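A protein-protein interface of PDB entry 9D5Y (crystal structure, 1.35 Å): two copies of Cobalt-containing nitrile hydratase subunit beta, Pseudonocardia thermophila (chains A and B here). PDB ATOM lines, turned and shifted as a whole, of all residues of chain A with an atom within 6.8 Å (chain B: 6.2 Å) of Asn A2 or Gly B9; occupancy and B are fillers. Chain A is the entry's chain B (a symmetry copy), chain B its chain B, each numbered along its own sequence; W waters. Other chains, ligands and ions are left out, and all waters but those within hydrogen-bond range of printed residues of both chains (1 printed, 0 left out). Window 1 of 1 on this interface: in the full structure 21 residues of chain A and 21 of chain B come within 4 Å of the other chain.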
ATOM      1  N   MET A   1      20.419  25.652  11.255  1.00  0.00           N
ATOM      2  CA  MET A   1      20.929  25.325   9.915  1.00  0.00           C
ATOM      3  C   MET A   1      20.271  26.181   8.828  1.00  0.00           C
ATOM      4  O   MET A   1      19.401  27.005   9.110  1.00  0.00           O
ATOM      5  CB  MET A   1      20.750  23.819   9.626  1.00  0.00           C
ATOM      6  CG  MET A   1      19.376  23.142  10.050  1.00  0.00           C
ATOM      7  SD  MET A   1      18.145  22.885   8.698  1.00  0.00           S
ATOM      8  CE  MET A   1      19.060  21.929   7.490  1.00  0.00           C
ATOM      9  N   ASN A   2      20.682  26.000   7.578  1.00  0.00           N
ATOM     10  CA  ASN A   2      20.110  26.790   6.490  1.00  0.00           C
ATOM     11  C   ASN A   2      19.120  25.983   5.652  1.00  0.00           C
ATOM     12  O   ASN A   2      19.371  25.736   4.467  1.00  0.00           O
ATOM     13  CB  ASN A   2      21.216  27.332   5.574  1.00  0.00           C
ATOM     14  CG  ASN A   2      22.033  28.439   6.228  1.00  0.00           C
ATOM     15  OD1 ASN A   2      21.815  28.783   7.392  1.00  0.00           O
ATOM     16  ND2 ASN A   2      22.961  29.015   5.480  1.00  0.00           N
ATOM     17  N   GLY A   3      17.997  25.573   6.250  1.00  0.00           N
ATOM     18  CA  GLY A   3      17.031  24.734   5.579  1.00  0.00           C
ATOM     19  C   GLY A   3      15.780  25.467   5.092  1.00  0.00           C
ATOM     20  O   GLY A   3      15.542  26.641   5.373  1.00  0.00           O
ATOM     21  N   VAL A   4      14.954  24.715   4.355  1.00  0.00           N
ATOM     22  CA  VAL A   4      13.764  25.262   3.701  1.00  0.00           C
ATOM     23  C   VAL A   4      12.696  25.655   4.708  1.00  0.00           C
ATOM     24  O   VAL A   4      11.832  26.489   4.422  1.00  0.00           O
ATOM     25  CB  VAL A   4      13.234  24.226   2.697  1.00  0.00           C
ATOM     26  CG1 VAL A   4      11.948  24.694   2.106  1.00  0.00           C
ATOM     27  CG2 VAL A   4      14.261  23.986   1.613  1.00  0.00           C
ATOM     28  N   TYR A   5      12.707  25.040   5.878  1.00  0.00           N
ATOM     29  CA  TYR A   5      11.786  25.432   6.925  1.00  0.00           C
ATOM     30  C   TYR A   5      11.917  26.919   7.262  1.00  0.00           C
ATOM     31  O   TYR A   5      10.963  27.526   7.765  1.00  0.00           O
ATOM     32  CB  TYR A   5      12.088  24.558   8.132  1.00  0.00           C
ATOM     33  CG  TYR A   5      13.343  24.997   8.825  1.00  0.00           C
ATOM     34  CD1 TYR A   5      13.299  26.010   9.772  1.00  0.00           C
ATOM     35  CD2 TYR A   5      14.569  24.438   8.522  1.00  0.00           C
ATOM     36  CE1 TYR A   5      14.414  26.449  10.394  1.00  0.00           C
ATOM     37  CE2 TYR A   5      15.704  24.876   9.151  1.00  0.00           C
ATOM     38  CZ  TYR A   5      15.612  25.889  10.089  1.00  0.00           C
ATOM     39  OH  TYR A   5      16.707  26.370  10.771  1.00  0.00           O
ATOM     40  N   ASP A   6      13.089  27.518   7.012  1.00  0.00           N
ATOM     41  CA  ASP A   6      13.360  28.930   7.314  1.00  0.00           C
ATOM     42  C   ASP A   6      12.818  29.756   6.146  1.00  0.00           C
ATOM     43  O   ASP A   6      13.535  30.186   5.241  1.00  0.00           O
ATOM     44  CB  ASP A   6      14.854  29.126   7.570  1.00  0.00           C
ATOM     45  CG  ASP A   6      15.261  30.589   7.758  1.00  0.00           C
ATOM     46  OD1 ASP A   6      14.386  31.451   7.976  1.00  0.00           O
ATOM     47  OD2 ASP A   6      16.485  30.868   7.699  1.00  0.00           O
ATOM     48  N   ALA A 150      26.774  34.601  11.314  1.00  0.00           N
ATOM     49  CA  ALA A 150      27.190  33.207  11.354  1.00  0.00           C
ATOM     50  C   ALA A 150      26.087  32.318  10.808  1.00  0.00           C
ATOM     51  O   ALA A 150      24.904  32.624  10.915  1.00  0.00           O
ATOM     52  CB  ALA A 150      27.508  32.780  12.779  1.00  0.00           C
ATOM     53  N   SER A 151      26.483  31.203  10.213  1.00  0.00           N
ATOM     54  CA  SER A 151      25.539  30.289   9.581  1.00  0.00           C
ATOM     55  C   SER A 151      25.822  28.886  10.074  1.00  0.00           C
ATOM     56  O   SER A 151      26.239  28.012   9.311  1.00  0.00           O
ATOM     57  CB  SER A 151      25.634  30.395   8.064  1.00  0.00           C
ATOM     58  OG  SER A 151      26.979  30.225   7.686  1.00  0.00           O
ATOM     59  N   PRO A 152      25.582  28.634  11.349  1.00  0.00           N
ATOM     60  CA  PRO A 152      25.940  27.337  11.920  1.00  0.00           C
ATOM     61  C   PRO A 152      25.157  26.241  11.229  1.00  0.00           C
ATOM     62  O   PRO A 152      24.068  26.461  10.698  1.00  0.00           O
ATOM     63  CB  PRO A 152      25.518  27.475  13.384  1.00  0.00           C
ATOM     64  CG  PRO A 152      24.381  28.466  13.320  1.00  0.00           C
ATOM     65  CD  PRO A 152      24.822  29.464  12.294  1.00  0.00           C
ATOM     66  N   LYS A 153      25.719  25.045  11.222  1.00  0.00           N
ATOM     67  CA  LYS A 153      24.995  23.966  10.574  1.00  0.00           C
ATOM     68  C   LYS A 153      24.017  23.260  11.487  1.00  0.00           C
ATOM     69  O   LYS A 153      23.069  22.647  10.985  1.00  0.00           O
ATOM     70  CB  LYS A 153      25.935  22.985   9.896  1.00  0.00           C
ATOM     71  CG  LYS A 153      26.525  23.615   8.683  1.00  0.00           C
ATOM     72  CD  LYS A 153      26.373  22.721   7.476  1.00  0.00           C
ATOM     73  CE  LYS A 153      26.370  23.599   6.239  1.00  0.00           C
ATOM     74  NZ  LYS A 153      27.256  24.795   6.461  1.00  0.00           N
ATOM     75  N   GLY A 154      24.203  23.349  12.798  1.00  0.00           N
ATOM     76  CA  GLY A 154      23.256  22.793  13.733  1.00  0.00           C
ATOM     77  C   GLY A 154      22.057  23.701  13.966  1.00  0.00           C
ATOM     78  O   GLY A 154      21.799  24.673  13.250  1.00  0.00           O
ATOM     79  N   ARG A 158      18.233  31.519  13.855  1.00  0.00           N
ATOM     80  CA  ARG A 158      18.862  32.602  13.118  1.00  0.00           C
ATOM     81  C   ARG A 158      18.244  32.664  11.731  1.00  0.00           C
ATOM     82  O   ARG A 158      18.896  32.294  10.764  1.00  0.00           O
ATOM     83  CB  ARG A 158      20.388  32.382  13.027  1.00  0.00           C
ATOM     84  CG  ARG A 158      21.079  32.221  14.354  1.00  0.00           C
ATOM     85  CD  ARG A 158      22.484  31.689  14.214  1.00  0.00           C
ATOM     86  NE  ARG A 158      23.136  31.646  15.518  1.00  0.00           N
ATOM     87  CZ  ARG A 158      23.976  32.567  15.967  1.00  0.00           C
ATOM     88  NH1 ARG A 158      24.301  33.625  15.237  1.00  0.00           N
ATOM     89  NH2 ARG A 158      24.497  32.430  17.177  1.00  0.00           N
ATOM     90  N   ARG A 160      17.304  33.544   8.118  1.00  0.00           N
ATOM     91  CA  ARG A 160      18.226  34.140   7.165  1.00  0.00           C
ATOM     92  C   ARG A 160      17.884  35.597   6.873  1.00  0.00           C
ATOM     93  O   ARG A 160      18.774  36.389   6.562  1.00  0.00           O
ATOM     94  CB  ARG A 160      18.220  33.333   5.885  1.00  0.00           C
ATOM     95  CG  ARG A 160      19.115  32.134   5.978  1.00  0.00           C
ATOM     96  CD  ARG A 160      19.187  31.415   4.669  1.00  0.00           C
ATOM     97  NE  ARG A 160      17.834  31.150   4.196  1.00  0.00           N
ATOM     98  CZ  ARG A 160      17.055  30.172   4.641  1.00  0.00           C
ATOM     99  NH1 ARG A 160      17.384  29.462   5.714  1.00  0.00           N
ATOM    100  NH2 ARG A 160      15.902  29.922   4.016  1.00  0.00           N
ATOM    101  N   ARG A 163      19.844  38.012   9.308  1.00  0.00           N
ATOM    102  CA  ARG A 163      21.268  37.912   9.531  1.00  0.00           C
ATOM    103  C   ARG A 163      21.982  39.123   8.957  1.00  0.00           C
ATOM    104  O   ARG A 163      21.694  39.566   7.839  1.00  0.00           O
ATOM    105  CB  ARG A 163      21.804  36.631   8.911  1.00  0.00           C
ATOM    106  CG  ARG A 163      21.207  35.383   9.514  1.00  0.00           C
ATOM    107  CD  ARG A 163      21.954  34.164   9.037  1.00  0.00           C
ATOM    108  NE  ARG A 163      21.201  32.948   9.298  1.00  0.00           N
ATOM    109  CZ  ARG A 163      21.483  31.761   8.776  1.00  0.00           C
ATOM    110  NH1 ARG A 163      22.503  31.590   7.947  1.00  0.00           N
ATOM    111  NH2 ARG A 163      20.727  30.714   9.106  1.00  0.00           N
ATOM    112  N   VAL B   7      18.966  28.556  -4.193  1.00  0.00           N
ATOM    113  CA  VAL B   7      19.374  27.563  -3.201  1.00  0.00           C
ATOM    114  C   VAL B   7      20.753  27.815  -2.607  1.00  0.00           C
ATOM    115  O   VAL B   7      21.122  27.136  -1.634  1.00  0.00           O
ATOM    116  CB  VAL B   7      19.289  26.127  -3.768  1.00  0.00           C
ATOM    117  CG1 VAL B   7      17.877  25.804  -4.170  1.00  0.00           C
ATOM    118  CG2 VAL B   7      20.229  25.966  -4.973  1.00  0.00           C
ATOM    119  N   GLY B   8      21.531  28.747  -3.155  1.00  0.00           N
ATOM    120  CA  GLY B   8      22.882  28.925  -2.673  1.00  0.00           C
ATOM    121  C   GLY B   8      22.915  29.195  -1.190  1.00  0.00           C
ATOM    122  O   GLY B   8      22.279  30.137  -0.716  1.00  0.00           O
ATOM    123  N   GLY B   9      23.656  28.375  -0.446  1.00  0.00           N
ATOM    124  CA  GLY B   9      23.728  28.487   0.993  1.00  0.00           C
ATOM    125  C   GLY B   9      22.720  27.653   1.747  1.00  0.00           C
ATOM    126  O   GLY B   9      22.795  27.594   2.978  1.00  0.00           O
ATOM    127  N   THR B  10      21.790  27.001   1.054  1.00  0.00           N
ATOM    128  CA  THR B  10      20.795  26.166   1.712  1.00  0.00           C
ATOM    129  C   THR B  10      21.425  24.901   2.287  1.00  0.00           C
ATOM    130  O   THR B  10      22.394  24.357   1.750  1.00  0.00           O
ATOM    131  CB  THR B  10      19.710  25.781   0.711  1.00  0.00           C
ATOM    132  OG1 THR B  10      19.017  26.958   0.290  1.00  0.00           O
ATOM    133  CG2 THR B  10      18.716  24.814   1.334  1.00  0.00           C
ATOM    134  N   ASP B  11      20.868  24.435   3.394  1.00  0.00           N
ATOM    135  CA  ASP B  11      21.305  23.181   3.976  1.00  0.00           C
ATOM    136  C   ASP B  11      20.184  22.157   3.861  1.00  0.00           C
ATOM    137  O   ASP B  11      19.029  22.482   3.564  1.00  0.00           O
ATOM    138  CB  ASP B  11      21.665  23.334   5.466  1.00  0.00           C
ATOM    139  CG  ASP B  11      22.841  24.264   5.714  1.00  0.00           C
ATOM    140  OD1 ASP B  11      23.816  24.234   4.931  1.00  0.00           O
ATOM    141  OD2 ASP B  11      22.835  24.957   6.754  1.00  0.00           O
ATOM    142  N   GLY B  12      20.534  20.908   4.147  1.00  0.00           N
ATOM    143  CA  GLY B  12      19.542  19.863   4.286  1.00  0.00           C
ATOM    144  C   GLY B  12      18.929  19.358   3.001  1.00  0.00           C
ATOM    145  O   GLY B  12      17.895  18.678   3.048  1.00  0.00           O
ATOM    146  N   TYR B 161      22.105  34.974  -0.751  1.00  0.00           N
ATOM    147  CA  TYR B 161      23.310  34.884   0.057  1.00  0.00           C
ATOM    148  C   TYR B 161      24.310  36.008  -0.196  1.00  0.00           C
ATOM    149  O   TYR B 161      25.238  36.154   0.608  1.00  0.00           O
ATOM    150  CB  TYR B 161      23.945  33.498  -0.083  1.00  0.00           C
ATOM    151  CG  TYR B 161      24.739  33.267  -1.345  1.00  0.00           C
ATOM    152  CD1 TYR B 161      24.133  32.807  -2.498  1.00  0.00           C
ATOM    153  CD2 TYR B 161      26.101  33.466  -1.366  1.00  0.00           C
ATOM    154  CE1 TYR B 161      24.862  32.585  -3.652  1.00  0.00           C
ATOM    155  CE2 TYR B 161      26.839  33.241  -2.510  1.00  0.00           C
ATOM    156  CZ  TYR B 161      26.218  32.797  -3.646  1.00  0.00           C
ATOM    157  OH  TYR B 161      26.988  32.576  -4.772  1.00  0.00           O
ATOM    158  N   TRP B 204      29.562  33.759   5.053  1.00  0.00           N
ATOM    159  CA  TRP B 204      29.014  32.748   5.949  1.00  0.00           C
ATOM    160  C   TRP B 204      29.273  32.995   7.426  1.00  0.00           C
ATOM    161  O   TRP B 204      28.795  32.210   8.254  1.00  0.00           O
ATOM    162  CB  TRP B 204      29.495  31.340   5.551  1.00  0.00           C
ATOM    163  CG  TRP B 204      29.412  31.135   4.082  1.00  0.00           C
ATOM    164  CD1 TRP B 204      30.448  31.012   3.204  1.00  0.00           C
ATOM    165  CD2 TRP B 204      28.218  31.071   3.303  1.00  0.00           C
ATOM    166  NE1 TRP B 204      29.969  30.877   1.930  1.00  0.00           N
ATOM    167  CE2 TRP B 204      28.602  30.908   1.966  1.00  0.00           C
ATOM    168  CE3 TRP B 204      26.862  31.144   3.609  1.00  0.00           C
ATOM    169  CZ2 TRP B 204      27.685  30.805   0.945  1.00  0.00           C
ATOM    170  CZ3 TRP B 204      25.961  31.052   2.596  1.00  0.00           C
ATOM    171  CH2 TRP B 204      26.371  30.879   1.280  1.00  0.00           C
HETATM  172  O   HOH W   1      16.419  22.129   3.634  1.00  0.00           O
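No position is printed for both chains.
ND2 of Asn A2 lies within hydrogen-bond range of O of Gly B9, 2.9 Å away. N of Asn A2 sits at hydrogen-bond distance from OD2 of Asp B11 (2.5 Å). OD1 of Asp B11 lies within salt-bridge range of NZ of Lys A153 (3.8 Å). The backbone carbonyl oxygen (O) of Trp B204 lies within hydrogen-bond range of the side-chain hydroxyl (OG) of Ser A151, at 2.7 Å.
Of the printed residues of chain B, Met A1 touches Asp B11 and Gly B12. Asn A2 touches just these residues of chain B: Gly B9 (2.9 Å), Thr B10 (3.1 Å) and Asp B11 (2.3 Å). Printed residues of chain B within 4 Å of Ala A150: Trp B204. Gly B9 touches one residue of chain A. Printed residues of chain A within 4 Å of Thr B10: Asn A2 (3.1 Å). Of the printed residues of chain A, Gly B12 touches Met A1 (3.8 Å). The nearest residue of chain B that does not touch Asn A2 is Trp B204 (4.6 Å). The nearest printed residue of chain B that does not touch Met A1 is Thr B10 (6.4 Å).
Water W1 bridges the backbone carbonyl oxygen of Asp B11 (2.6 Å) and the backbone NH of Val A4 (3.1 Å).
The backbone carbonyl oxygen of Val B7 is in hydrogen-bond range of the side-chain hydroxyl of Thr B10. N of Gly A3 lies close to SD of Met A1 (3.6 Å). The side-chain hydroxyl (OH) of Tyr A5 sits at hydrogen-bond distance from the backbone carbonyl oxygen (O) of Met A1 (3.2 Å). N of Met A1 is in hydrogen-bond range of O of Gly A154 (2.6 Å). OD1 of Asn A2 lies within hydrogen-bond range of NH2 of Arg A163 (2.8 Å). O of Gly A3 is in hydrogen-bond range of NH1 of Arg A160.
Asp B11 touches Met A1 (OD2 to C, 3.5 Å). CE of Met A1 touches N of Gly B12, at 3.8 Å. Thr B10 touches Asn A2 (C to O, 3.1 Å). Gly A3 touches Asp B11 (CA to O, 3.6 Å). Ala A150 touches Trp B204 (CA to O, 3.6 Å).
Of the 14 printed residues of chain A, 6 touch a printed residue of chain B. Hydrophobic or aromatic side chains of chain A within 4 Å of the printed part of chain B: Met A1. Among the printed residues, 9 pairs touch across the chains.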
